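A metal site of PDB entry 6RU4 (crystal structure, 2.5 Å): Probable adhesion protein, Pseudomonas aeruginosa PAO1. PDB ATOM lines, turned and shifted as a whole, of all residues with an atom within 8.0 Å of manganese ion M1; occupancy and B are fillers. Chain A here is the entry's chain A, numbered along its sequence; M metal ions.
ND1 of His 111 sits at hydrogen-bond distance from O of Gly 178 (3.5 Å).
A ring nitrogen (ND1) of His 111 lies within hydrogen-bond range of the side-chain amide oxygen (OD1) of Asn 109 (2.7 Å).
The side-chain carboxylate (OE1) of Glu 196 sits at hydrogen-bond distance from a ring nitrogen (ND1) of His 177, at 3.1 Å.
OD1 of Asn 39 sits at hydrogen-bond distance from ND1 of His 41 (3.1 Å).
Manganese ion M1 is bound by a ring nitrogen (NE2) of His 199 (2.2 Å), a ring nitrogen (NE2) of His 250 (2.2 Å), a ring nitrogen (NE2) of His 111 (2.3 Å), a ring nitrogen (NE2) of His 177 (2.3 Å), a ring nitrogen (NE2) of His 66 (2.4 Å) and a ring nitrogen (NE2) of His 41 (2.5 Å).
Of the 21 residues printed, 6 come within 4 Å of manganese ion M1.
The nearest printed residue that does not touch manganese ion M1 is Ala 179 (4.8 Å).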
ATOM      1  N   LEU A  13     -25.288  -4.854 -11.297  1.00  0.00           N
ATOM      2  CA  LEU A  13     -25.373  -5.706 -10.107  1.00  0.00           C
ATOM      3  C   LEU A  13     -26.084  -4.976  -8.968  1.00  0.00           C
ATOM      4  O   LEU A  13     -25.987  -3.758  -8.901  1.00  0.00           O
ATOM      5  CB  LEU A  13     -23.951  -6.150  -9.667  1.00  0.00           C
ATOM      6  CG  LEU A  13     -23.011  -6.751 -10.757  1.00  0.00           C
ATOM      7  CD1 LEU A  13     -21.582  -6.491 -10.483  1.00  0.00           C
ATOM      8  CD2 LEU A  13     -23.257  -8.201 -10.995  1.00  0.00           C
ATOM      9  N   ASN A  39     -29.536 -14.518 -12.097  1.00  0.00           N
ATOM     10  CA  ASN A  39     -28.208 -14.799 -11.585  1.00  0.00           C
ATOM     11  C   ASN A  39     -27.297 -14.113 -12.585  1.00  0.00           C
ATOM     12  O   ASN A  39     -27.380 -14.391 -13.798  1.00  0.00           O
ATOM     13  CB  ASN A  39     -27.907 -16.300 -11.546  1.00  0.00           C
ATOM     14  CG  ASN A  39     -26.538 -16.634 -11.011  1.00  0.00           C
ATOM     15  OD1 ASN A  39     -25.934 -15.890 -10.251  1.00  0.00           O
ATOM     16  ND2 ASN A  39     -26.017 -17.790 -11.389  1.00  0.00           N
ATOM     17  N   PRO A  40     -26.465 -13.159 -12.111  1.00  0.00           N
ATOM     18  CA  PRO A  40     -25.574 -12.469 -13.040  1.00  0.00           C
ATOM     19  C   PRO A  40     -24.531 -13.339 -13.732  1.00  0.00           C
ATOM     20  O   PRO A  40     -24.031 -12.956 -14.793  1.00  0.00           O
ATOM     21  CB  PRO A  40     -24.921 -11.420 -12.162  1.00  0.00           C
ATOM     22  CG  PRO A  40     -25.004 -11.996 -10.776  1.00  0.00           C
ATOM     23  CD  PRO A  40     -26.295 -12.665 -10.728  1.00  0.00           C
ATOM     24  N   HIS A  41     -24.216 -14.518 -13.143  1.00  0.00           N
ATOM     25  CA  HIS A  41     -23.223 -15.453 -13.652  1.00  0.00           C
ATOM     26  C   HIS A  41     -23.772 -16.231 -14.825  1.00  0.00           C
ATOM     27  O   HIS A  41     -23.033 -16.600 -15.738  1.00  0.00           O
ATOM     28  CB  HIS A  41     -22.791 -16.419 -12.539  1.00  0.00           C
ATOM     29  CG  HIS A  41     -22.167 -15.733 -11.371  1.00  0.00           C
ATOM     30  ND1 HIS A  41     -22.920 -15.379 -10.268  1.00  0.00           N
ATOM     31  CD2 HIS A  41     -20.894 -15.329 -11.176  1.00  0.00           C
ATOM     32  CE1 HIS A  41     -22.082 -14.790  -9.430  1.00  0.00           C
ATOM     33  NE2 HIS A  41     -20.846 -14.737  -9.932  1.00  0.00           N
ATOM     34  N   GLY A  65     -14.673  -7.258 -14.597  1.00  0.00           N
ATOM     35  CA  GLY A  65     -14.968  -8.669 -14.824  1.00  0.00           C
ATOM     36  C   GLY A  65     -16.291  -9.233 -14.337  1.00  0.00           C
ATOM     37  O   GLY A  65     -16.586 -10.404 -14.611  1.00  0.00           O
ATOM     38  N   HIS A  66     -17.115  -8.435 -13.622  1.00  0.00           N
ATOM     39  CA  HIS A  66     -18.384  -8.957 -13.120  1.00  0.00           C
ATOM     40  C   HIS A  66     -19.616  -8.463 -13.856  1.00  0.00           C
ATOM     41  O   HIS A  66     -20.732  -8.680 -13.382  1.00  0.00           O
ATOM     42  CB  HIS A  66     -18.537  -8.725 -11.609  1.00  0.00           C
ATOM     43  CG  HIS A  66     -19.138  -9.909 -10.917  1.00  0.00           C
ATOM     44  ND1 HIS A  66     -20.306 -10.522 -11.390  1.00  0.00           N
ATOM     45  CD2 HIS A  66     -18.695 -10.599  -9.850  1.00  0.00           C
ATOM     46  CE1 HIS A  66     -20.533 -11.531 -10.581  1.00  0.00           C
ATOM     47  NE2 HIS A  66     -19.593 -11.621  -9.641  1.00  0.00           N
ATOM     48  N   ASN A 109      -9.722 -10.273  -9.522  1.00  0.00           N
ATOM     49  CA  ASN A 109     -10.902 -10.581  -8.732  1.00  0.00           C
ATOM     50  C   ASN A 109     -11.876  -9.393  -8.919  1.00  0.00           C
ATOM     51  O   ASN A 109     -11.552  -8.266  -8.516  1.00  0.00           O
ATOM     52  CB  ASN A 109     -10.546 -10.749  -7.243  1.00  0.00           C
ATOM     53  CG  ASN A 109     -11.672 -11.354  -6.416  1.00  0.00           C
ATOM     54  OD1 ASN A 109     -12.839 -11.265  -6.770  1.00  0.00           O
ATOM     55  ND2 ASN A 109     -11.365 -11.984  -5.308  1.00  0.00           N
ATOM     56  N   PRO A 110     -13.081  -9.595  -9.528  1.00  0.00           N
ATOM     57  CA  PRO A 110     -13.977  -8.451  -9.768  1.00  0.00           C
ATOM     58  C   PRO A 110     -14.902  -8.067  -8.621  1.00  0.00           C
ATOM     59  O   PRO A 110     -15.666  -7.123  -8.767  1.00  0.00           O
ATOM     60  CB  PRO A 110     -14.793  -8.900 -10.994  1.00  0.00           C
ATOM     61  CG  PRO A 110     -14.326 -10.339 -11.316  1.00  0.00           C
ATOM     62  CD  PRO A 110     -13.633 -10.835 -10.121  1.00  0.00           C
ATOM     63  N   HIS A 111     -14.822  -8.751  -7.489  1.00  0.00           N
ATOM     64  CA  HIS A 111     -15.708  -8.573  -6.328  1.00  0.00           C
ATOM     65  C   HIS A 111     -15.285  -7.492  -5.379  1.00  0.00           C
ATOM     66  O   HIS A 111     -15.375  -7.666  -4.155  1.00  0.00           O
ATOM     67  CB  HIS A 111     -15.865  -9.897  -5.578  1.00  0.00           C
ATOM     68  CG  HIS A 111     -16.327 -11.005  -6.462  1.00  0.00           C
ATOM     69  ND1 HIS A 111     -15.440 -11.674  -7.291  1.00  0.00           N
ATOM     70  CD2 HIS A 111     -17.561 -11.482  -6.669  1.00  0.00           C
ATOM     71  CE1 HIS A 111     -16.144 -12.588  -7.911  1.00  0.00           C
ATOM     72  NE2 HIS A 111     -17.439 -12.530  -7.547  1.00  0.00           N
ATOM     73  N   PHE A 113     -16.838  -4.804  -4.864  1.00  0.00           N
ATOM     74  CA  PHE A 113     -18.090  -4.463  -4.211  1.00  0.00           C
ATOM     75  C   PHE A 113     -18.331  -5.247  -2.886  1.00  0.00           C
ATOM     76  O   PHE A 113     -19.207  -4.854  -2.134  1.00  0.00           O
ATOM     77  CB  PHE A 113     -19.263  -4.599  -5.187  1.00  0.00           C
ATOM     78  CG  PHE A 113     -19.369  -5.925  -5.906  1.00  0.00           C
ATOM     79  CD1 PHE A 113     -20.022  -7.009  -5.302  1.00  0.00           C
ATOM     80  CD2 PHE A 113     -18.947  -6.055  -7.224  1.00  0.00           C
ATOM     81  CE1 PHE A 113     -20.176  -8.227  -5.987  1.00  0.00           C
ATOM     82  CE2 PHE A 113     -19.127  -7.263  -7.921  1.00  0.00           C
ATOM     83  CZ  PHE A 113     -19.746  -8.336  -7.307  1.00  0.00           C
ATOM     84  N   LEU A 114     -17.541  -6.304  -2.556  1.00  0.00           N
ATOM     85  CA  LEU A 114     -17.726  -7.044  -1.293  1.00  0.00           C
ATOM     86  C   LEU A 114     -16.722  -6.622  -0.214  1.00  0.00           C
ATOM     87  O   LEU A 114     -16.566  -7.308   0.804  1.00  0.00           O
ATOM     88  CB  LEU A 114     -17.758  -8.574  -1.502  1.00  0.00           C
ATOM     89  CG  LEU A 114     -19.035  -9.115  -2.182  1.00  0.00           C
ATOM     90  CD1 LEU A 114     -18.896 -10.554  -2.519  1.00  0.00           C
ATOM     91  CD2 LEU A 114     -20.250  -8.919  -1.319  1.00  0.00           C
ATOM     92  N   HIS A 177     -17.175 -19.966  -3.815  1.00  0.00           N
ATOM     93  CA  HIS A 177     -17.129 -18.889  -4.805  1.00  0.00           C
ATOM     94  C   HIS A 177     -16.042 -17.903  -4.382  1.00  0.00           C
ATOM     95  O   HIS A 177     -15.985 -17.558  -3.214  1.00  0.00           O
ATOM     96  CB  HIS A 177     -18.514 -18.191  -4.818  1.00  0.00           C
ATOM     97  CG  HIS A 177     -18.783 -17.354  -6.029  1.00  0.00           C
ATOM     98  ND1 HIS A 177     -19.371 -17.893  -7.165  1.00  0.00           N
ATOM     99  CD2 HIS A 177     -18.538 -16.044  -6.235  1.00  0.00           C
ATOM    100  CE1 HIS A 177     -19.434 -16.898  -8.034  1.00  0.00           C
ATOM    101  NE2 HIS A 177     -18.950 -15.759  -7.518  1.00  0.00           N
ATOM    102  N   GLY A 178     -15.205 -17.463  -5.331  1.00  0.00           N
ATOM    103  CA  GLY A 178     -14.102 -16.533  -5.081  1.00  0.00           C
ATOM    104  C   GLY A 178     -14.474 -15.083  -4.980  1.00  0.00           C
ATOM    105  O   GLY A 178     -13.816 -14.214  -5.555  1.00  0.00           O
ATOM    106  N   ALA A 179     -15.510 -14.790  -4.207  1.00  0.00           N
ATOM    107  CA  ALA A 179     -16.047 -13.454  -3.985  1.00  0.00           C
ATOM    108  C   ALA A 179     -15.554 -12.714  -2.718  1.00  0.00           C
ATOM    109  O   ALA A 179     -15.747 -11.490  -2.597  1.00  0.00           O
ATOM    110  CB  ALA A 179     -17.569 -13.554  -3.941  1.00  0.00           C
ATOM    111  N   TYR A 180     -14.971 -13.438  -1.751  1.00  0.00           N
ATOM    112  CA  TYR A 180     -14.761 -12.849  -0.435  1.00  0.00           C
ATOM    113  C   TYR A 180     -13.322 -12.486  -0.033  1.00  0.00           C
ATOM    114  O   TYR A 180     -13.084 -12.105   1.118  1.00  0.00           O
ATOM    115  CB  TYR A 180     -15.403 -13.779   0.603  1.00  0.00           C
ATOM    116  CG  TYR A 180     -16.831 -14.108   0.203  1.00  0.00           C
ATOM    117  CD1 TYR A 180     -17.813 -13.126   0.253  1.00  0.00           C
ATOM    118  CD2 TYR A 180     -17.162 -15.349  -0.318  1.00  0.00           C
ATOM    119  CE1 TYR A 180     -19.126 -13.399  -0.155  1.00  0.00           C
ATOM    120  CE2 TYR A 180     -18.471 -15.635  -0.742  1.00  0.00           C
ATOM    121  CZ  TYR A 180     -19.442 -14.658  -0.647  1.00  0.00           C
ATOM    122  OH  TYR A 180     -20.741 -14.919  -1.024  1.00  0.00           O
ATOM    123  N   GLU A 196     -14.319 -23.372  -6.505  1.00  0.00           N
ATOM    124  CA  GLU A 196     -14.623 -23.145  -7.914  1.00  0.00           C
ATOM    125  C   GLU A 196     -13.309 -22.918  -8.677  1.00  0.00           C
ATOM    126  O   GLU A 196     -12.527 -22.054  -8.285  1.00  0.00           O
ATOM    127  CB  GLU A 196     -15.544 -21.931  -8.071  1.00  0.00           C
ATOM    128  CG  GLU A 196     -17.014 -22.242  -7.800  1.00  0.00           C
ATOM    129  CD  GLU A 196     -17.995 -21.143  -8.111  1.00  0.00           C
ATOM    130  OE1 GLU A 196     -17.547 -20.025  -8.473  1.00  0.00           O
ATOM    131  OE2 GLU A 196     -19.212 -21.386  -7.984  1.00  0.00           O
ATOM    132  N   HIS A 199     -14.108 -18.313 -11.905  1.00  0.00           N
ATOM    133  CA  HIS A 199     -15.292 -17.548 -11.532  1.00  0.00           C
ATOM    134  C   HIS A 199     -16.603 -18.081 -12.109  1.00  0.00           C
ATOM    135  O   HIS A 199     -16.798 -18.062 -13.334  1.00  0.00           O
ATOM    136  CB  HIS A 199     -15.117 -16.067 -11.860  1.00  0.00           C
ATOM    137  CG  HIS A 199     -16.200 -15.189 -11.299  1.00  0.00           C
ATOM    138  ND1 HIS A 199     -16.662 -14.084 -12.000  1.00  0.00           N
ATOM    139  CD2 HIS A 199     -16.863 -15.282 -10.124  1.00  0.00           C
ATOM    140  CE1 HIS A 199     -17.582 -13.551 -11.225  1.00  0.00           C
ATOM    141  NE2 HIS A 199     -17.764 -14.256 -10.092  1.00  0.00           N
ATOM    142  N   GLY A 200     -17.472 -18.573 -11.229  1.00  0.00           N
ATOM    143  CA  GLY A 200     -18.786 -19.105 -11.576  1.00  0.00           C
ATOM    144  C   GLY A 200     -18.798 -20.459 -12.267  1.00  0.00           C
ATOM    145  O   GLY A 200     -19.818 -20.834 -12.833  1.00  0.00           O
ATOM    146  N   GLU A 226     -22.388 -20.211  -0.460  1.00  0.00           N
ATOM    147  CA  GLU A 226     -23.329 -19.230  -0.993  1.00  0.00           C
ATOM    148  C   GLU A 226     -24.746 -19.310  -0.441  1.00  0.00           C
ATOM    149  O   GLU A 226     -25.318 -20.396  -0.361  1.00  0.00           O
ATOM    150  CB  GLU A 226     -23.388 -19.338  -2.527  1.00  0.00           C
ATOM    151  CG  GLU A 226     -22.167 -18.823  -3.252  1.00  0.00           C
ATOM    152  CD  GLU A 226     -21.830 -17.371  -2.985  1.00  0.00           C
ATOM    153  OE1 GLU A 226     -22.698 -16.491  -3.205  1.00  0.00           O
ATOM    154  OE2 GLU A 226     -20.697 -17.112  -2.525  1.00  0.00           O
ATOM    155  N   HIS A 250     -23.490 -12.792  -1.722  1.00  0.00           N
ATOM    156  CA  HIS A 250     -22.801 -12.181  -2.848  1.00  0.00           C
ATOM    157  C   HIS A 250     -23.540 -10.879  -3.231  1.00  0.00           C
ATOM    158  O   HIS A 250     -23.025 -10.084  -4.021  1.00  0.00           O
ATOM    159  CB  HIS A 250     -22.774 -13.194  -4.016  1.00  0.00           C
ATOM    160  CG  HIS A 250     -21.933 -12.854  -5.220  1.00  0.00           C
ATOM    161  ND1 HIS A 250     -22.235 -11.777  -6.034  1.00  0.00           N
ATOM    162  CD2 HIS A 250     -20.931 -13.554  -5.797  1.00  0.00           C
ATOM    163  CE1 HIS A 250     -21.388 -11.831  -7.045  1.00  0.00           C
ATOM    164  NE2 HIS A 250     -20.577 -12.878  -6.949  1.00  0.00           N
ATOM    165  N   SER A 252     -26.690 -10.561  -4.765  1.00  0.00           N
ATOM    166  CA  SER A 252     -27.099 -10.784  -6.177  1.00  0.00           C
ATOM    167  C   SER A 252     -28.496 -11.433  -6.308  1.00  0.00           C
ATOM    168  O   SER A 252     -28.958 -11.762  -7.415  1.00  0.00           O
ATOM    169  CB  SER A 252     -26.074 -11.650  -6.901  1.00  0.00           C
ATOM    170  OG  SER A 252     -26.185 -13.021  -6.530  1.00  0.00           O
HETATM  171 MN    MN M   1     -19.143 -13.698  -8.464  1.00  0.00          MN
HETATM  172 MN    MN M   2     -12.584 -15.121  -8.777  1.00  0.00          MN
